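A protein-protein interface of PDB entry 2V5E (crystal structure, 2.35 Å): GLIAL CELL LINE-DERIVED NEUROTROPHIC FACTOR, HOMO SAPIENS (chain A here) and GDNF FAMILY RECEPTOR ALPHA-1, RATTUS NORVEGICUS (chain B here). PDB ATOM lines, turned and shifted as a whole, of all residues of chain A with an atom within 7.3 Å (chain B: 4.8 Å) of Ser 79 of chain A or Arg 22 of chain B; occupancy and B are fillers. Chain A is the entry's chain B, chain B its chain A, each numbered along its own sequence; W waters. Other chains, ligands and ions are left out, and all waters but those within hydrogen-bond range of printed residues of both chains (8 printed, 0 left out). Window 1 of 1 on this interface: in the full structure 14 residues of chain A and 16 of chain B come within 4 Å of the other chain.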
ATOM      1  N   VAL A  17      23.883   3.951   2.600  1.00  0.00           N
ATOM      2  CA  VAL A  17      23.988   2.803   3.498  1.00  0.00           C
ATOM      3  C   VAL A  17      24.368   3.272   4.920  1.00  0.00           C
ATOM      4  O   VAL A  17      23.977   2.657   5.917  1.00  0.00           O
ATOM      5  CB  VAL A  17      24.979   1.732   2.961  1.00  0.00           C
ATOM      6  CG1 VAL A  17      25.297   0.675   4.014  1.00  0.00           C
ATOM      7  CG2 VAL A  17      24.417   1.056   1.704  1.00  0.00           C
ATOM      8  N   GLU A  28      28.264   3.816  -0.562  1.00  0.00           N
ATOM      9  CA  GLU A  28      27.195   3.176  -1.350  1.00  0.00           C
ATOM     10  C   GLU A  28      25.781   3.510  -0.843  1.00  0.00           C
ATOM     11  O   GLU A  28      25.615   4.020   0.270  1.00  0.00           O
ATOM     12  CB  GLU A  28      27.434   1.664  -1.472  1.00  0.00           C
ATOM     13  CG  GLU A  28      28.688   1.319  -2.297  1.00  0.00           C
ATOM     14  CD  GLU A  28      28.488   0.134  -3.230  1.00  0.00           C
ATOM     15  OE1 GLU A  28      27.369  -0.033  -3.755  1.00  0.00           O
ATOM     16  OE2 GLU A  28      29.453  -0.635  -3.439  1.00  0.00           O
ATOM     17  N   GLU A  29      24.779   3.216  -1.673  1.00  0.00           N
ATOM     18  CA  GLU A  29      23.394   3.690  -1.489  1.00  0.00           C
ATOM     19  C   GLU A  29      22.388   2.547  -1.662  1.00  0.00           C
ATOM     20  O   GLU A  29      22.745   1.484  -2.145  1.00  0.00           O
ATOM     21  CB  GLU A  29      23.081   4.818  -2.494  1.00  0.00           C
ATOM     22  CG  GLU A  29      24.151   5.929  -2.544  1.00  0.00           C
ATOM     23  CD  GLU A  29      23.770   7.155  -3.378  1.00  0.00           C
ATOM     24  OE1 GLU A  29      22.627   7.254  -3.886  1.00  0.00           O
ATOM     25  OE2 GLU A  29      24.640   8.035  -3.528  1.00  0.00           O
ATOM     26  N   ASP A  76      15.197  -8.352  -2.127  1.00  0.00           N
ATOM     27  CA  ASP A  76      16.406  -9.145  -2.331  1.00  0.00           C
ATOM     28  C   ASP A  76      17.584  -8.522  -1.601  1.00  0.00           C
ATOM     29  O   ASP A  76      17.564  -7.323  -1.272  1.00  0.00           O
ATOM     30  CB  ASP A  76      16.747  -9.255  -3.828  1.00  0.00           C
ATOM     31  CG  ASP A  76      15.646  -9.945  -4.653  1.00  0.00           C
ATOM     32  OD1 ASP A  76      15.070 -10.952  -4.206  1.00  0.00           O
ATOM     33  OD2 ASP A  76      15.372  -9.470  -5.763  1.00  0.00           O
ATOM     34  N   ASP A  77      18.606  -9.344  -1.363  1.00  0.00           N
ATOM     35  CA  ASP A  77      19.833  -8.921  -0.710  1.00  0.00           C
ATOM     36  C   ASP A  77      20.466  -7.732  -1.421  1.00  0.00           C
ATOM     37  O   ASP A  77      20.402  -7.620  -2.641  1.00  0.00           O
ATOM     38  CB  ASP A  77      20.851 -10.065  -0.655  1.00  0.00           C
ATOM     39  CG  ASP A  77      20.296 -11.331  -0.021  1.00  0.00           C
ATOM     40  OD1 ASP A  77      19.263 -11.270   0.695  1.00  0.00           O
ATOM     41  OD2 ASP A  77      20.909 -12.403  -0.245  1.00  0.00           O
ATOM     42  N   LEU A  78      21.060  -6.845  -0.628  1.00  0.00           N
ATOM     43  CA  LEU A  78      21.808  -5.695  -1.123  1.00  0.00           C
ATOM     44  C   LEU A  78      23.265  -5.810  -0.681  1.00  0.00           C
ATOM     45  O   LEU A  78      23.557  -6.027   0.494  1.00  0.00           O
ATOM     46  CB  LEU A  78      21.225  -4.395  -0.580  1.00  0.00           C
ATOM     47  CG  LEU A  78      22.005  -3.163  -1.023  1.00  0.00           C
ATOM     48  CD1 LEU A  78      21.191  -2.413  -2.071  1.00  0.00           C
ATOM     49  CD2 LEU A  78      22.333  -2.273   0.190  1.00  0.00           C
ATOM     50  N   SER A  79      24.175  -5.663  -1.628  1.00  0.00           N
ATOM     51  CA  SER A  79      25.592  -5.759  -1.337  1.00  0.00           C
ATOM     52  C   SER A  79      26.260  -4.440  -1.692  1.00  0.00           C
ATOM     53  O   SER A  79      25.697  -3.632  -2.439  1.00  0.00           O
ATOM     54  CB  SER A  79      26.223  -6.929  -2.110  1.00  0.00           C
ATOM     55  OG  SER A  79      26.134  -6.685  -3.499  1.00  0.00           O
ATOM     56  N   PHE A  80      27.448  -4.220  -1.140  1.00  0.00           N
ATOM     57  CA  PHE A  80      28.207  -2.993  -1.388  1.00  0.00           C
ATOM     58  C   PHE A  80      29.660  -3.217  -0.996  1.00  0.00           C
ATOM     59  O   PHE A  80      29.964  -4.120  -0.212  1.00  0.00           O
ATOM     60  CB  PHE A  80      27.615  -1.806  -0.603  1.00  0.00           C
ATOM     61  CG  PHE A  80      27.450  -2.072   0.867  1.00  0.00           C
ATOM     62  CD1 PHE A  80      26.299  -2.694   1.350  1.00  0.00           C
ATOM     63  CD2 PHE A  80      28.445  -1.706   1.768  1.00  0.00           C
ATOM     64  CE1 PHE A  80      26.148  -2.970   2.723  1.00  0.00           C
ATOM     65  CE2 PHE A  80      28.307  -1.974   3.158  1.00  0.00           C
ATOM     66  CZ  PHE A  80      27.155  -2.605   3.625  1.00  0.00           C
ATOM     67  N   LEU A  81      30.545  -2.397  -1.568  1.00  0.00           N
ATOM     68  CA  LEU A  81      31.969  -2.397  -1.261  1.00  0.00           C
ATOM     69  C   LEU A  81      32.232  -1.196  -0.353  1.00  0.00           C
ATOM     70  O   LEU A  81      31.879  -0.076  -0.707  1.00  0.00           O
ATOM     71  CB  LEU A  81      32.775  -2.260  -2.570  1.00  0.00           C
ATOM     72  CG  LEU A  81      34.309  -2.263  -2.526  1.00  0.00           C
ATOM     73  CD1 LEU A  81      34.846  -3.677  -2.356  1.00  0.00           C
ATOM     74  CD2 LEU A  81      34.866  -1.636  -3.792  1.00  0.00           C
ATOM     75  N   ASP A  82      32.848  -1.430   0.805  1.00  0.00           N
ATOM     76  CA  ASP A  82      33.088  -0.350   1.770  1.00  0.00           C
ATOM     77  C   ASP A  82      34.397   0.407   1.503  1.00  0.00           C
ATOM     78  O   ASP A  82      35.067   0.168   0.485  1.00  0.00           O
ATOM     79  CB  ASP A  82      32.969  -0.848   3.227  1.00  0.00           C
ATOM     80  CG  ASP A  82      34.189  -1.637   3.706  1.00  0.00           C
ATOM     81  OD1 ASP A  82      35.254  -1.609   3.052  1.00  0.00           O
ATOM     82  OD2 ASP A  82      34.090  -2.283   4.770  1.00  0.00           O
ATOM     83  N   TYR A  87      33.707  -6.191   1.084  1.00  0.00           N
ATOM     84  CA  TYR A  87      32.321  -6.409   0.652  1.00  0.00           C
ATOM     85  C   TYR A  87      31.443  -6.826   1.814  1.00  0.00           C
ATOM     86  O   TYR A  87      31.873  -7.562   2.706  1.00  0.00           O
ATOM     87  CB  TYR A  87      32.231  -7.502  -0.433  1.00  0.00           C
ATOM     88  CG  TYR A  87      32.459  -7.007  -1.836  1.00  0.00           C
ATOM     89  CD1 TYR A  87      31.542  -6.140  -2.453  1.00  0.00           C
ATOM     90  CD2 TYR A  87      33.589  -7.390  -2.551  1.00  0.00           C
ATOM     91  CE1 TYR A  87      31.752  -5.669  -3.739  1.00  0.00           C
ATOM     92  CE2 TYR A  87      33.807  -6.924  -3.850  1.00  0.00           C
ATOM     93  CZ  TYR A  87      32.882  -6.076  -4.438  1.00  0.00           C
ATOM     94  OH  TYR A  87      33.091  -5.624  -5.732  1.00  0.00           O
ATOM     95  N   HIS A  88      30.197  -6.376   1.769  1.00  0.00           N
ATOM     96  CA  HIS A  88      29.187  -6.793   2.733  1.00  0.00           C
ATOM     97  C   HIS A  88      27.891  -7.092   2.021  1.00  0.00           C
ATOM     98  O   HIS A  88      27.660  -6.600   0.908  1.00  0.00           O
ATOM     99  CB  HIS A  88      28.948  -5.687   3.767  1.00  0.00           C
ATOM    100  CG  HIS A  88      30.191  -5.248   4.466  1.00  0.00           C
ATOM    101  ND1 HIS A  88      30.662  -5.867   5.606  1.00  0.00           N
ATOM    102  CD2 HIS A  88      31.090  -4.283   4.156  1.00  0.00           C
ATOM    103  CE1 HIS A  88      31.787  -5.282   5.983  1.00  0.00           C
ATOM    104  NE2 HIS A  88      32.065  -4.316   5.121  1.00  0.00           N
ATOM    105  N   ILE A  89      27.042  -7.885   2.668  1.00  0.00           N
ATOM    106  CA  ILE A  89      25.693  -8.124   2.165  1.00  0.00           C
ATOM    107  C   ILE A  89      24.662  -7.898   3.254  1.00  0.00           C
ATOM    108  O   ILE A  89      24.764  -8.467   4.331  1.00  0.00           O
ATOM    109  CB  ILE A  89      25.509  -9.549   1.561  1.00  0.00           C
ATOM    110  CG1 ILE A  89      26.452  -9.773   0.388  1.00  0.00           C
ATOM    111  CG2 ILE A  89      24.069  -9.750   1.062  1.00  0.00           C
ATOM    112  CD1 ILE A  89      27.498 -10.761   0.690  1.00  0.00           C
ATOM    113  N   LEU A  90      23.690  -7.048   2.947  1.00  0.00           N
ATOM    114  CA  LEU A  90      22.499  -6.838   3.756  1.00  0.00           C
ATOM    115  C   LEU A  90      21.388  -7.786   3.347  1.00  0.00           C
ATOM    116  O   LEU A  90      21.058  -7.896   2.167  1.00  0.00           O
ATOM    117  CB  LEU A  90      21.992  -5.414   3.571  1.00  0.00           C
ATOM    118  CG  LEU A  90      22.422  -4.332   4.559  1.00  0.00           C
ATOM    119  CD1 LEU A  90      21.912  -2.993   4.066  1.00  0.00           C
ATOM    120  CD2 LEU A  90      21.877  -4.625   5.954  1.00  0.00           C
ATOM    121  N   HIS A  93      16.450  -6.605   5.097  1.00  0.00           N
ATOM    122  CA  HIS A  93      16.619  -5.232   5.545  1.00  0.00           C
ATOM    123  C   HIS A  93      15.514  -4.310   5.019  1.00  0.00           C
ATOM    124  O   HIS A  93      15.347  -3.196   5.515  1.00  0.00           O
ATOM    125  CB  HIS A  93      17.983  -4.711   5.077  1.00  0.00           C
ATOM    126  CG  HIS A  93      18.113  -4.602   3.589  1.00  0.00           C
ATOM    127  ND1 HIS A  93      18.214  -5.706   2.768  1.00  0.00           N
ATOM    128  CD2 HIS A  93      18.152  -3.521   2.772  1.00  0.00           C
ATOM    129  CE1 HIS A  93      18.300  -5.309   1.509  1.00  0.00           C
ATOM    130  NE2 HIS A  93      18.264  -3.988   1.483  1.00  0.00           N
ATOM    131  N   ALA B   9      27.781   1.586  -9.233  1.00  0.00           N
ATOM    132  CA  ALA B   9      27.301   0.846  -8.052  1.00  0.00           C
ATOM    133  C   ALA B   9      25.953   1.362  -7.537  1.00  0.00           C
ATOM    134  O   ALA B   9      25.080   0.568  -7.176  1.00  0.00           O
ATOM    135  CB  ALA B   9      28.337   0.851  -6.937  1.00  0.00           C
ATOM    136  N   CYS B  12      23.249   0.317 -10.062  1.00  0.00           N
ATOM    137  CA  CYS B  12      23.018  -1.111  -9.943  1.00  0.00           C
ATOM    138  C   CYS B  12      22.124  -1.461  -8.742  1.00  0.00           C
ATOM    139  O   CYS B  12      21.155  -2.201  -8.900  1.00  0.00           O
ATOM    140  CB  CYS B  12      24.345  -1.850  -9.856  1.00  0.00           C
ATOM    141  SG  CYS B  12      24.146  -3.590  -9.679  1.00  0.00           S
ATOM    142  N   ASN B  13      22.454  -0.928  -7.558  1.00  0.00           N
ATOM    143  CA  ASN B  13      21.698  -1.183  -6.321  1.00  0.00           C
ATOM    144  C   ASN B  13      20.289  -0.609  -6.321  1.00  0.00           C
ATOM    145  O   ASN B  13      19.444  -1.031  -5.512  1.00  0.00           O
ATOM    146  CB  ASN B  13      22.468  -0.670  -5.102  1.00  0.00           C
ATOM    147  CG  ASN B  13      23.599  -1.590  -4.689  1.00  0.00           C
ATOM    148  OD1 ASN B  13      23.811  -2.658  -5.280  1.00  0.00           O
ATOM    149  ND2 ASN B  13      24.333  -1.183  -3.665  1.00  0.00           N
ATOM    150  N   CYS B  18      19.943  -5.747 -11.437  1.00  0.00           N
ATOM    151  CA  CYS B  18      21.376  -5.639 -11.184  1.00  0.00           C
ATOM    152  C   CYS B  18      21.667  -5.924  -9.709  1.00  0.00           C
ATOM    153  O   CYS B  18      22.539  -6.742  -9.389  1.00  0.00           O
ATOM    154  CB  CYS B  18      21.926  -4.276 -11.609  1.00  0.00           C
ATOM    155  SG  CYS B  18      23.728  -4.201 -11.580  1.00  0.00           S
ATOM    156  N   LYS B  19      20.906  -5.281  -8.822  1.00  0.00           N
ATOM    157  CA  LYS B  19      21.061  -5.451  -7.375  1.00  0.00           C
ATOM    158  C   LYS B  19      21.079  -6.919  -6.924  1.00  0.00           C
ATOM    159  O   LYS B  19      21.980  -7.338  -6.189  1.00  0.00           O
ATOM    160  CB  LYS B  19      19.953  -4.698  -6.645  1.00  0.00           C
ATOM    161  CG  LYS B  19      20.025  -4.799  -5.122  1.00  0.00           C
ATOM    162  CD  LYS B  19      18.755  -4.268  -4.505  1.00  0.00           C
ATOM    163  CE  LYS B  19      17.621  -5.224  -4.748  1.00  0.00           C
ATOM    164  NZ  LYS B  19      16.307  -4.577  -4.489  1.00  0.00           N
ATOM    165  N   LYS B  20      20.079  -7.678  -7.377  1.00  0.00           N
ATOM    166  CA  LYS B  20      19.905  -9.088  -7.047  1.00  0.00           C
ATOM    167  C   LYS B  20      21.066  -9.966  -7.534  1.00  0.00           C
ATOM    168  O   LYS B  20      21.588 -10.791  -6.790  1.00  0.00           O
ATOM    169  CB  LYS B  20      18.583  -9.577  -7.664  1.00  0.00           C
ATOM    170  CG  LYS B  20      18.261 -11.062  -7.452  1.00  0.00           C
ATOM    171  CD  LYS B  20      16.856 -11.411  -7.947  1.00  0.00           C
ATOM    172  CE  LYS B  20      16.800 -11.479  -9.472  1.00  0.00           C
ATOM    173  NZ  LYS B  20      15.483 -11.013 -10.017  1.00  0.00           N
ATOM    174  N   TYR B  21      21.458  -9.787  -8.790  1.00  0.00           N
ATOM    175  CA  TYR B  21      22.518 -10.599  -9.386  1.00  0.00           C
ATOM    176  C   TYR B  21      23.916 -10.187  -8.924  1.00  0.00           C
ATOM    177  O   TYR B  21      24.822 -11.017  -8.898  1.00  0.00           O
ATOM    178  CB  TYR B  21      22.415 -10.597 -10.921  1.00  0.00           C
ATOM    179  CG  TYR B  21      21.329 -11.508 -11.470  1.00  0.00           C
ATOM    180  CD1 TYR B  21      21.573 -12.866 -11.686  1.00  0.00           C
ATOM    181  CD2 TYR B  21      20.069 -11.016 -11.768  1.00  0.00           C
ATOM    182  CE1 TYR B  21      20.562 -13.718 -12.183  1.00  0.00           C
ATOM    183  CE2 TYR B  21      19.062 -11.841 -12.271  1.00  0.00           C
ATOM    184  CZ  TYR B  21      19.313 -13.189 -12.473  1.00  0.00           C
ATOM    185  OH  TYR B  21      18.317 -13.999 -12.963  1.00  0.00           O
ATOM    186  N   ARG B  22      24.095  -8.918  -8.561  1.00  0.00           N
ATOM    187  CA  ARG B  22      25.316  -8.504  -7.844  1.00  0.00           C
ATOM    188  C   ARG B  22      25.431  -9.261  -6.497  1.00  0.00           C
ATOM    189  O   ARG B  22      26.453  -9.914  -6.238  1.00  0.00           O
ATOM    190  CB  ARG B  22      25.352  -6.984  -7.628  1.00  0.00           C
ATOM    191  CG  ARG B  22      26.655  -6.448  -7.033  1.00  0.00           C
ATOM    192  CD  ARG B  22      26.536  -4.956  -6.688  1.00  0.00           C
ATOM    193  NE  ARG B  22      27.818  -4.352  -6.291  1.00  0.00           N
ATOM    194  CZ  ARG B  22      27.924  -3.211  -5.606  1.00  0.00           C
ATOM    195  NH1 ARG B  22      26.829  -2.540  -5.233  1.00  0.00           N
ATOM    196  NH2 ARG B  22      29.119  -2.732  -5.290  1.00  0.00           N
ATOM    197  N   SER B  23      24.392  -9.193  -5.652  1.00  0.00           N
ATOM    198  CA  SER B  23      24.427  -9.916  -4.359  1.00  0.00           C
ATOM    199  C   SER B  23      24.613 -11.411  -4.573  1.00  0.00           C
ATOM    200  O   SER B  23      25.328 -12.055  -3.813  1.00  0.00           O
ATOM    201  CB  SER B  23      23.169  -9.659  -3.524  1.00  0.00           C
ATOM    202  OG  SER B  23      23.024  -8.264  -3.307  1.00  0.00           O
ATOM    203  N   ALA B  24      23.967 -11.945  -5.611  1.00  0.00           N
ATOM    204  CA  ALA B  24      24.069 -13.356  -5.977  1.00  0.00           C
ATOM    205  C   ALA B  24      25.505 -13.797  -6.276  1.00  0.00           C
ATOM    206  O   ALA B  24      25.818 -14.972  -6.125  1.00  0.00           O
ATOM    207  CB  ALA B  24      23.148 -13.678  -7.170  1.00  0.00           C
ATOM    208  N   TYR B  25      26.369 -12.876  -6.704  1.00  0.00           N
ATOM    209  CA  TYR B  25      27.771 -13.236  -6.918  1.00  0.00           C
ATOM    210  C   TYR B  25      28.696 -12.792  -5.794  1.00  0.00           C
ATOM    211  O   TYR B  25      29.653 -13.495  -5.462  1.00  0.00           O
ATOM    212  CB  TYR B  25      28.286 -12.843  -8.326  1.00  0.00           C
ATOM    213  CG  TYR B  25      28.833 -11.430  -8.529  1.00  0.00           C
ATOM    214  CD1 TYR B  25      28.091 -10.475  -9.192  1.00  0.00           C
ATOM    215  CD2 TYR B  25      30.132 -11.088  -8.127  1.00  0.00           C
ATOM    216  CE1 TYR B  25      28.601  -9.198  -9.407  1.00  0.00           C
ATOM    217  CE2 TYR B  25      30.652  -9.824  -8.360  1.00  0.00           C
ATOM    218  CZ  TYR B  25      29.878  -8.885  -8.974  1.00  0.00           C
ATOM    219  OH  TYR B  25      30.364  -7.620  -9.188  1.00  0.00           O
ATOM    220  N   ILE B  26      28.408 -11.643  -5.187  1.00  0.00           N
ATOM    221  CA  ILE B  26      29.175 -11.228  -4.005  1.00  0.00           C
ATOM    222  C   ILE B  26      29.114 -12.292  -2.900  1.00  0.00           C
ATOM    223  O   ILE B  26      30.126 -12.555  -2.229  1.00  0.00           O
ATOM    224  CB  ILE B  26      28.728  -9.861  -3.458  1.00  0.00           C
ATOM    225  CG1 ILE B  26      28.954  -8.766  -4.510  1.00  0.00           C
ATOM    226  CG2 ILE B  26      29.496  -9.515  -2.186  1.00  0.00           C
ATOM    227  CD1 ILE B  26      30.391  -8.722  -5.032  1.00  0.00           C
ATOM    228  N   PHE B  50      25.739 -13.111 -13.641  1.00  0.00           N
ATOM    229  CA  PHE B  50      25.688 -11.641 -13.581  1.00  0.00           C
ATOM    230  C   PHE B  50      25.793 -10.987 -14.958  1.00  0.00           C
ATOM    231  O   PHE B  50      24.948 -10.181 -15.337  1.00  0.00           O
ATOM    232  CB  PHE B  50      26.758 -11.054 -12.641  1.00  0.00           C
ATOM    233  CG  PHE B  50      26.690  -9.534 -12.509  1.00  0.00           C
ATOM    234  CD1 PHE B  50      25.711  -8.929 -11.717  1.00  0.00           C
ATOM    235  CD2 PHE B  50      27.588  -8.721 -13.189  1.00  0.00           C
ATOM    236  CE1 PHE B  50      25.637  -7.525 -11.593  1.00  0.00           C
ATOM    237  CE2 PHE B  50      27.536  -7.332 -13.062  1.00  0.00           C
ATOM    238  CZ  PHE B  50      26.562  -6.732 -12.263  1.00  0.00           C
ATOM    239  N   MET B  62      29.862  -0.965 -14.082  1.00  0.00           N
ATOM    240  CA  MET B  62      30.744  -1.312 -12.988  1.00  0.00           C
ATOM    241  C   MET B  62      32.094  -1.876 -13.442  1.00  0.00           C
ATOM    242  O   MET B  62      33.112  -1.678 -12.765  1.00  0.00           O
ATOM    243  CB  MET B  62      30.037  -2.299 -12.070  1.00  0.00           C
ATOM    244  CG  MET B  62      28.728  -1.755 -11.532  1.00  0.00           C
ATOM    245  SD  MET B  62      28.116  -2.778 -10.200  1.00  0.00           S
ATOM    246  CE  MET B  62      29.276  -2.400  -8.897  1.00  0.00           C
ATOM    247  N   ARG B  75      38.321   0.349  -6.695  1.00  0.00           N
ATOM    248  CA  ARG B  75      36.936  -0.099  -6.678  1.00  0.00           C
ATOM    249  C   ARG B  75      36.635  -0.932  -7.937  1.00  0.00           C
ATOM    250  O   ARG B  75      36.065  -2.030  -7.851  1.00  0.00           O
ATOM    251  CB  ARG B  75      35.986   1.110  -6.552  1.00  0.00           C
ATOM    252  CG  ARG B  75      34.530   0.798  -6.824  1.00  0.00           C
ATOM    253  CD  ARG B  75      33.644   1.970  -6.486  1.00  0.00           C
ATOM    254  NE  ARG B  75      33.371   2.053  -5.055  1.00  0.00           N
ATOM    255  CZ  ARG B  75      32.383   1.412  -4.432  1.00  0.00           C
ATOM    256  NH1 ARG B  75      31.555   0.621  -5.102  1.00  0.00           N
ATOM    257  NH2 ARG B  75      32.238   1.551  -3.122  1.00  0.00           N
HETATM  258  O   HOH W   1      32.646   3.112  -0.113  1.00  0.00           O
HETATM  259  O   HOH W   2      22.200 -12.727  -2.620  1.00  0.00           O
HETATM  260  O   HOH W   3      30.101  -5.734  -7.293  1.00  0.00           O
HETATM  261  O   HOH W   4      15.768  -7.081  -6.551  1.00  0.00           O
HETATM  262  O   HOH W   5      25.723   1.945  -4.171  1.00  0.00           O
HETATM  263  O   HOH W   6      16.577  -4.794  -1.811  1.00  0.00           O
HETATM  264  O   HOH W   7      13.896  -6.516  -4.323  1.00  0.00           O
HETATM  265  O   HOH W   8      23.619  -5.471  -4.564  1.00  0.00           O
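OD1 of Asn 13 of chain B lies within hydrogen-bond range of NH1 of Arg 22 of chain B.
OG of Ser 23 of chain B lies within hydrogen-bond range of O of Lys 19 of chain B (3.2 Å).
O of Glu 28 of chain A lies within hydrogen-bond range of N of Val 17 of chain A (2.9 Å).
OE2 of Glu 28 of chain A sits at hydrogen-bond distance from N of Leu 81 of chain A (2.8 Å).
The backbone carbonyl oxygen of Leu 78 of chain A sits at hydrogen-bond distance from the backbone NH of Leu 90 of chain A (2.7 Å).
The side-chain sulfur (SG) of Cys 12 of chain B forms a disulfide with the side-chain sulfur (SG) of Cys 18 of chain B (2.0 Å).
Water W4 lies within hydrogen-bond range of OD2 of Asp 76 of chain A (2.5 Å) and NZ of Lys 19 of chain B (3.3 Å).
Water W5 lies within hydrogen-bond range of OE1 of Glu 28 of chain A (2.6 Å), N of Glu 29 of chain A (3.0 Å), O of Ala 9 of chain B (3.4 Å) and ND2 of Asn 13 of chain B (3.5 Å).
Water W3 lies within hydrogen-bond range of the side-chain hydroxyl of Tyr 25 of chain B, the guanidinium group of Arg 22 of chain B and the side-chain hydroxyl of Tyr 87 of chain A.
Water W6 lies within hydrogen-bond range of the side-chain amino group (NZ) of Lys 19 of chain B (2.7 Å) and the backbone carbonyl oxygen (O) of Asp 76 of chain A (2.8 Å).
Water W8 lies within hydrogen-bond range of OD1 of Asn 13 of chain B (2.9 Å), O of Lys 19 of chain B (3.0 Å), OG of Ser 79 of chain A (3.0 Å) and OG of Ser 23 of chain B (3.1 Å).
Water W7 bridges NZ of Lys 19 of chain B and N of Asp 76 of chain A.
Of the printed residues of chain B, Asp 77 of chain A touches Lys 19 and Ser 23.
Ser 79 of chain A touches just these residues of chain B: Asn 13, Arg 22, Ser 23 and Ile 26.
Of the printed residues of chain A, Asn 13 of chain B touches Glu 28, Glu 29, Leu 78 and Ser 79.
Of the printed residues of chain A, Arg 22 of chain B touches Glu 28 (2.8 Å), Ser 79 (3.2 Å) and Leu 81 (3.9999 Å).
Of the printed residues of chain A, Ser 23 of chain B touches Asp 77, Leu 78 and Ser 79.
The nearest printed residue of chain B that does not touch Ser 79 of chain A is Lys 19 of chain B (5.0 Å).
The nearest printed residue of chain A that does not touch Ser 23 of chain B is Ile 89 of chain A (4.7 Å).
The side-chain carboxylate (OE1) of Glu 28 of chain A lies within hydrogen-bond range of the side-chain amide nitrogen (ND2) of Asn 13 of chain B (3.2 Å).
The side-chain amide nitrogen (ND2) of Asn 13 of chain B is in hydrogen-bond range of the backbone carbonyl oxygen (O) of Glu 29 of chain A (3.5 Å).
The side-chain amide nitrogen (ND2) of Asn 13 of chain B sits at hydrogen-bond distance from the backbone carbonyl oxygen (O) of Ser 79 of chain A.
The side-chain carboxylate (OE2) of Glu 28 of chain A is in salt-bridge range of the guanidinium group (NH2) of Arg 22 of chain B, at 2.8 Å.
NH1 of Arg 22 of chain B is in hydrogen-bond range of O of Ser 79 of chain A.
OG of Ser 23 of chain B lies within hydrogen-bond range of O of Asp 77 of chain A.
OG of Ser 23 of chain B sits at hydrogen-bond distance from N of Ser 79 of chain A (3.3 Å).
The guanidinium group (NH1) of Arg 75 of chain B is in salt-bridge range of the side-chain carboxylate (OE2) of Glu 28 of chain A, at 3.0 Å.
The backbone carbonyl oxygen of Leu 81 of chain A is in hydrogen-bond range of the guanidinium group of Arg 75 of chain B (2.9 Å).
Hydrophobic or aromatic side chains of chain B that line the printed part of chain A: Ala 9 and Ile 26.
Of the 15 printed residues of chain A, 9 touch a printed residue of chain B.
Hydrophobic or aromatic side chains of chain A within 4 Å of the printed part of chain B: Leu 78, Leu 81, Tyr 87 and Ile 89.
Among the printed residues, 19 pairs touch across the chains.
Among the printed residues, Asp or Glu carboxylates within 4 Å of a Lys or Arg side-chain nitrogen of the other chain: Glu 28 of chain A with Arg 22 of chain B and Glu 28 of chain A with Arg 75 of chain B.
Glu 28 of chain A touches Ala 9 of chain B (OE1 to CB, 3.4 Å).
OD2 of Asp 76 of chain A touches CD of Lys 20 of chain B, at 3.3 Å.
Asp 77 of chain A touches Lys 19 of chain B (O to CG, 3.8 Å).
Leu 78 of chain A touches Asn 13 of chain B (CD1 to CG, 3.7 Å).
CD1 of Leu 78 of chain A touches CD of Lys 19 of chain B, 3.9 Å away.
Ser 23 of chain B touches Leu 78 of chain A (OG to CA, 3.6 Å).
Ile 26 of chain B touches Ser 79 of chain A.
N of Leu 81 of chain A touches NH2 of Arg 22 of chain B (3.9999 Å).
Tyr 87 of chain A touches Ile 26 of chain B (CE1 to CD1, 3.6 Å).
Ile 89 of chain A touches Ile 26 of chain B (CD1 to CG2, 3.7 Å).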
